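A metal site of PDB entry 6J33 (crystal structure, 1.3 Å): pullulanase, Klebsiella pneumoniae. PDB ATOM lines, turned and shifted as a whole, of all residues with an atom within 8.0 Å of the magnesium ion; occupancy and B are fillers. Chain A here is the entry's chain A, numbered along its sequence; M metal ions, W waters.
The nearest printed residue that does not touch the magnesium ion is Ser 974 (4.1 Å).
O of Ser 974 sits close to OE1 of Gln 1040, 3.5 Å away. The backbone NH of Gln 1040 lies within hydrogen-bond range of the backbone carbonyl oxygen of Arg 975, 2.7 Å away. The side-chain carboxylate (OD2) of Asp 973 lies within salt-bridge range of the guanidinium group (NH1) of Arg 975 (2.7 Å). N of Asp 964 is in hydrogen-bond range of O of Asp 977, 2.9 Å away. The side-chain carboxylate (OD1) of Asp 964 sits at hydrogen-bond distance from the backbone NH (N) of Leu 972 (2.7 Å). The backbone carbonyl oxygen (O) of Asp 964 is in hydrogen-bond range of the side-chain amide nitrogen (NE2) of Gln 1044, at 2.9 Å. NH1 of Arg 943 is in salt-bridge range of OD1 of Asp 964 (2.9 Å). NE2 of Gln 1044 sits close to N of Ser 971 (3.3 Å).
The magnesium ion is bound by the side-chain amide oxygen of Gln 1040 (2.0 Å), the backbone carbonyl oxygen of Asp 973 (2.0 Å), the side-chain carboxylate of Asp 964 (2.1 Å), water W1 (2.1 Å), the backbone carbonyl oxygen of Val 976 (2.1 Å) and the side-chain hydroxyl of Ser 971 (2.2 Å).
Water W1 lies within hydrogen-bond range of O of Asp 964 (2.6 Å) and OD1 of Asp 977 (2.7 Å).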
ATOM      1  N   SER A 929      14.924 -34.168  21.059  1.00  0.00           N
ATOM      2  CA  SER A 929      16.279 -33.829  21.458  1.00  0.00           C
ATOM      3  C   SER A 929      17.187 -34.996  21.096  1.00  0.00           C
ATOM      4  O   SER A 929      16.787 -36.153  21.279  1.00  0.00           O
ATOM      5  CB  SER A 929      16.367 -33.592  22.962  1.00  0.00           C
ATOM      6  OG  SER A 929      17.711 -33.360  23.349  1.00  0.00           O
ATOM      7  N   LEU A 931      19.378 -35.900  22.947  1.00  0.00           N
ATOM      8  CA  LEU A 931      19.759 -36.474  24.234  1.00  0.00           C
ATOM      9  C   LEU A 931      19.002 -37.754  24.566  1.00  0.00           C
ATOM     10  O   LEU A 931      19.495 -38.544  25.368  1.00  0.00           O
ATOM     11  CB  LEU A 931      19.536 -35.439  25.341  1.00  0.00           C
ATOM     12  CG  LEU A 931      20.463 -34.213  25.263  1.00  0.00           C
ATOM     13  CD1 LEU A 931      20.023 -33.162  26.266  1.00  0.00           C
ATOM     14  CD2 LEU A 931      21.893 -34.630  25.522  1.00  0.00           C
ATOM     15  N   ARG A 943      26.341 -39.446  30.675  1.00  0.00           N
ATOM     16  CA  ARG A 943      25.290 -38.472  30.725  1.00  0.00           C
ATOM     17  C   ARG A 943      23.982 -38.819  31.430  1.00  0.00           C
ATOM     18  O   ARG A 943      23.304 -37.938  31.865  1.00  0.00           O
ATOM     19  CB  ARG A 943      24.940 -38.047  29.302  1.00  0.00           C
ATOM     20  CG  ARG A 943      26.055 -37.363  28.534  1.00  0.00           C
ATOM     21  CD  ARG A 943      25.709 -37.108  27.090  1.00  0.00           C
ATOM     22  NE  ARG A 943      26.798 -36.454  26.380  1.00  0.00           N
ATOM     23  CZ  ARG A 943      26.812 -35.186  26.018  1.00  0.00           C
ATOM     24  NH1 ARG A 943      25.855 -34.373  26.353  1.00  0.00           N
ATOM     25  NH2 ARG A 943      27.829 -34.723  25.358  1.00  0.00           N
ATOM     26  N   ASP A 963      22.416 -35.410  30.914  1.00  0.00           N
ATOM     27  CA  ASP A 963      23.281 -34.243  31.015  1.00  0.00           C
ATOM     28  C   ASP A 963      23.689 -33.735  29.635  1.00  0.00           C
ATOM     29  O   ASP A 963      24.094 -34.506  28.766  1.00  0.00           O
ATOM     30  CB  ASP A 963      24.518 -34.602  31.825  1.00  0.00           C
ATOM     31  CG  ASP A 963      25.361 -33.389  32.200  1.00  0.00           C
ATOM     32  OD1 ASP A 963      24.839 -32.246  32.168  1.00  0.00           O
ATOM     33  OD2 ASP A 963      26.546 -33.591  32.530  1.00  0.00           O
ATOM     34  N   ASP A 964      23.578 -32.413  29.446  1.00  0.00           N
ATOM     35  CA  ASP A 964      24.226 -31.740  28.335  1.00  0.00           C
ATOM     36  C   ASP A 964      25.205 -30.670  28.797  1.00  0.00           C
ATOM     37  O   ASP A 964      25.639 -29.833  27.991  1.00  0.00           O
ATOM     38  CB  ASP A 964      23.197 -31.148  27.358  1.00  0.00           C
ATOM     39  CG  ASP A 964      23.717 -31.107  25.920  1.00  0.00           C
ATOM     40  OD1 ASP A 964      24.485 -32.005  25.520  1.00  0.00           O
ATOM     41  OD2 ASP A 964      23.335 -30.154  25.202  1.00  0.00           O
ATOM     42  N   GLY A 965      25.574 -30.670  30.084  1.00  0.00           N
ATOM     43  CA  GLY A 965      26.431 -29.648  30.629  1.00  0.00           C
ATOM     44  C   GLY A 965      27.914 -29.917  30.412  1.00  0.00           C
ATOM     45  O   GLY A 965      28.324 -30.908  29.806  1.00  0.00           O
ATOM     46  N   ALA A 970      30.764 -32.113  25.011  1.00  0.00           N
ATOM     47  CA  ALA A 970      30.166 -31.101  24.161  1.00  0.00           C
ATOM     48  C   ALA A 970      28.667 -31.027  24.399  1.00  0.00           C
ATOM     49  O   ALA A 970      28.030 -31.997  24.837  1.00  0.00           O
ATOM     50  CB  ALA A 970      30.431 -31.416  22.688  1.00  0.00           C
ATOM     51  N   SER A 971      28.096 -29.857  24.139  1.00  0.00           N
ATOM     52  CA  SER A 971      26.654 -29.732  24.073  1.00  0.00           C
ATOM     53  C   SER A 971      26.172 -30.428  22.810  1.00  0.00           C
ATOM     54  O   SER A 971      26.580 -30.070  21.708  1.00  0.00           O
ATOM     55  CB  SER A 971      26.267 -28.250  24.031  1.00  0.00           C
ATOM     56  OG  SER A 971      24.884 -28.091  23.766  1.00  0.00           O
ATOM     57  N   LEU A 972      25.323 -31.445  22.982  1.00  0.00           N
ATOM     58  CA  LEU A 972      24.721 -32.126  21.846  1.00  0.00           C
ATOM     59  C   LEU A 972      23.378 -31.529  21.458  1.00  0.00           C
ATOM     60  O   LEU A 972      22.869 -31.845  20.372  1.00  0.00           O
ATOM     61  CB  LEU A 972      24.545 -33.615  22.144  1.00  0.00           C
ATOM     62  CG  LEU A 972      25.803 -34.358  22.542  1.00  0.00           C
ATOM     63  CD1 LEU A 972      25.464 -35.768  22.990  1.00  0.00           C
ATOM     64  CD2 LEU A 972      26.785 -34.385  21.378  1.00  0.00           C
ATOM     65  N   ASP A 973      22.796 -30.683  22.301  1.00  0.00           N
ATOM     66  CA  ASP A 973      21.540 -30.006  22.029  1.00  0.00           C
ATOM     67  C   ASP A 973      21.742 -28.536  22.364  1.00  0.00           C
ATOM     68  O   ASP A 973      21.964 -28.182  23.523  1.00  0.00           O
ATOM     69  CB  ASP A 973      20.410 -30.593  22.880  1.00  0.00           C
ATOM     70  CG  ASP A 973      19.034 -30.044  22.504  1.00  0.00           C
ATOM     71  OD1 ASP A 973      18.936 -28.862  22.105  1.00  0.00           O
ATOM     72  OD2 ASP A 973      18.049 -30.805  22.598  1.00  0.00           O
ATOM     73  N   SER A 974      21.640 -27.679  21.349  1.00  0.00           N
ATOM     74  CA  SER A 974      21.911 -26.259  21.540  1.00  0.00           C
ATOM     75  C   SER A 974      20.824 -25.554  22.346  1.00  0.00           C
ATOM     76  O   SER A 974      21.049 -24.431  22.810  1.00  0.00           O
ATOM     77  CB  SER A 974      22.067 -25.568  20.180  1.00  0.00           C
ATOM     78  OG  SER A 974      20.872 -25.651  19.437  1.00  0.00           O
ATOM     79  N   ARG A 975      19.654 -26.169  22.512  1.00  0.00           N
ATOM     80  CA  ARG A 975      18.561 -25.535  23.246  1.00  0.00           C
ATOM     81  C   ARG A 975      18.618 -25.778  24.742  1.00  0.00           C
ATOM     82  O   ARG A 975      18.107 -24.962  25.511  1.00  0.00           O
ATOM     83  CB  ARG A 975      17.206 -26.055  22.748  1.00  0.00           C
ATOM     84  CG  ARG A 975      16.971 -25.956  21.260  1.00  0.00           C
ATOM     85  CD  ARG A 975      15.745 -26.784  20.875  1.00  0.00           C
ATOM     86  NE  ARG A 975      15.897 -28.181  21.276  1.00  0.00           N
ATOM     87  CZ  ARG A 975      15.235 -28.762  22.268  1.00  0.00           C
ATOM     88  NH1 ARG A 975      15.461 -30.044  22.537  1.00  0.00           N
ATOM     89  NH2 ARG A 975      14.350 -28.090  22.986  1.00  0.00           N
ATOM     90  N   VAL A 976      19.206 -26.885  25.175  1.00  0.00           N
ATOM     91  CA  VAL A 976      19.140 -27.302  26.573  1.00  0.00           C
ATOM     92  C   VAL A 976      20.519 -27.695  27.100  1.00  0.00           C
ATOM     93  O   VAL A 976      21.386 -28.160  26.356  1.00  0.00           O
ATOM     94  CB  VAL A 976      18.144 -28.464  26.798  1.00  0.00           C
ATOM     95  CG1 VAL A 976      16.744 -28.088  26.309  1.00  0.00           C
ATOM     96  CG2 VAL A 976      18.624 -29.742  26.130  1.00  0.00           C
ATOM     97  N   ASP A 977      20.697 -27.510  28.409  1.00  0.00           N
ATOM     98  CA  ASP A 977      21.835 -28.033  29.147  1.00  0.00           C
ATOM     99  C   ASP A 977      21.531 -29.368  29.818  1.00  0.00           C
ATOM    100  O   ASP A 977      22.428 -29.960  30.439  1.00  0.00           O
ATOM    101  CB  ASP A 977      22.302 -27.028  30.197  1.00  0.00           C
ATOM    102  CG  ASP A 977      22.957 -25.792  29.583  1.00  0.00           C
ATOM    103  OD1 ASP A 977      23.749 -25.946  28.634  1.00  0.00           O
ATOM    104  OD2 ASP A 977      22.686 -24.685  30.072  1.00  0.00           O
ATOM    105  N   GLY A 978      20.296 -29.838  29.741  1.00  0.00           N
ATOM    106  CA  GLY A 978      19.948 -31.119  30.322  1.00  0.00           C
ATOM    107  C   GLY A 978      18.457 -31.347  30.227  1.00  0.00           C
ATOM    108  O   GLY A 978      17.683 -30.408  30.001  1.00  0.00           O
ATOM    109  N   LEU A1038      16.435 -27.909  30.989  1.00  0.00           N
ATOM    110  CA  LEU A1038      17.236 -26.788  31.464  1.00  0.00           C
ATOM    111  C   LEU A1038      17.596 -25.960  30.229  1.00  0.00           C
ATOM    112  O   LEU A1038      18.419 -26.400  29.427  1.00  0.00           O
ATOM    113  CB  LEU A1038      18.511 -27.287  32.132  1.00  0.00           C
ATOM    114  CG  LEU A1038      18.467 -27.924  33.516  1.00  0.00           C
ATOM    115  CD1 LEU A1038      19.866 -28.354  33.919  1.00  0.00           C
ATOM    116  CD2 LEU A1038      17.907 -26.945  34.544  1.00  0.00           C
ATOM    117  N   PRO A1039      17.010 -24.780  30.049  1.00  0.00           N
ATOM    118  CA  PRO A1039      17.276 -24.018  28.820  1.00  0.00           C
ATOM    119  C   PRO A1039      18.723 -23.570  28.764  1.00  0.00           C
ATOM    120  O   PRO A1039      19.314 -23.182  29.781  1.00  0.00           O
ATOM    121  CB  PRO A1039      16.325 -22.812  28.934  1.00  0.00           C
ATOM    122  CG  PRO A1039      15.390 -23.138  30.034  1.00  0.00           C
ATOM    123  CD  PRO A1039      16.086 -24.073  30.953  1.00  0.00           C
ATOM    124  N   GLN A1040      19.303 -23.624  27.573  1.00  0.00           N
ATOM    125  CA  GLN A1040      20.695 -23.281  27.388  1.00  0.00           C
ATOM    126  C   GLN A1040      20.810 -21.790  27.096  1.00  0.00           C
ATOM    127  O   GLN A1040      20.107 -21.259  26.226  1.00  0.00           O
ATOM    128  CB  GLN A1040      21.317 -24.099  26.247  1.00  0.00           C
ATOM    129  CG  GLN A1040      22.821 -23.936  26.117  1.00  0.00           C
ATOM    130  CD  GLN A1040      23.441 -24.973  25.203  1.00  0.00           C
ATOM    131  OE1 GLN A1040      22.983 -26.124  25.148  1.00  0.00           O
ATOM    132  NE2 GLN A1040      24.485 -24.594  24.474  1.00  0.00           N
ATOM    133  N   GLY A1041      21.676 -21.114  27.854  1.00  0.00           N
ATOM    134  CA  GLY A1041      21.868 -19.686  27.702  1.00  0.00           C
ATOM    135  C   GLY A1041      22.886 -19.305  26.639  1.00  0.00           C
ATOM    136  O   GLY A1041      22.965 -19.949  25.596  1.00  0.00           O
ATOM    137  N   SER A1043      26.115 -19.559  26.696  1.00  0.00           N
ATOM    138  CA  SER A1043      27.107 -20.612  26.561  1.00  0.00           C
ATOM    139  C   SER A1043      26.618 -21.848  27.287  1.00  0.00           C
ATOM    140  O   SER A1043      25.661 -21.798  28.072  1.00  0.00           O
ATOM    141  CB  SER A1043      28.478 -20.172  27.097  1.00  0.00           C
ATOM    142  OG  SER A1043      28.981 -19.060  26.379  1.00  0.00           O
ATOM    143  N   GLN A1044      27.273 -22.985  27.009  1.00  0.00           N
ATOM    144  CA  GLN A1044      26.911 -24.241  27.636  1.00  0.00           C
ATOM    145  C   GLN A1044      26.994 -24.116  29.154  1.00  0.00           C
ATOM    146  O   GLN A1044      27.960 -23.543  29.690  1.00  0.00           O
ATOM    147  CB  GLN A1044      27.852 -25.345  27.169  1.00  0.00           C
ATOM    148  CG  GLN A1044      27.678 -26.693  27.867  1.00  0.00           C
ATOM    149  CD  GLN A1044      28.731 -27.711  27.438  1.00  0.00           C
ATOM    150  OE1 GLN A1044      29.883 -27.355  27.191  1.00  0.00           O
ATOM    151  NE2 GLN A1044      28.340 -28.974  27.352  1.00  0.00           N
ATOM    152  N   GLY A1045      25.980 -24.639  29.852  1.00  0.00           N
ATOM    153  CA  GLY A1045      25.844 -24.470  31.272  1.00  0.00           C
ATOM    154  C   GLY A1045      26.291 -25.678  32.077  1.00  0.00           C
ATOM    155  O   GLY A1045      26.930 -26.612  31.573  1.00  0.00           O
HETATM  156 MG    MG M   1      23.148 -28.077  25.154  1.00  0.00          MG
HETATM  157  O   HOH W   1      24.395 -27.810  26.827  1.00  0.00           O
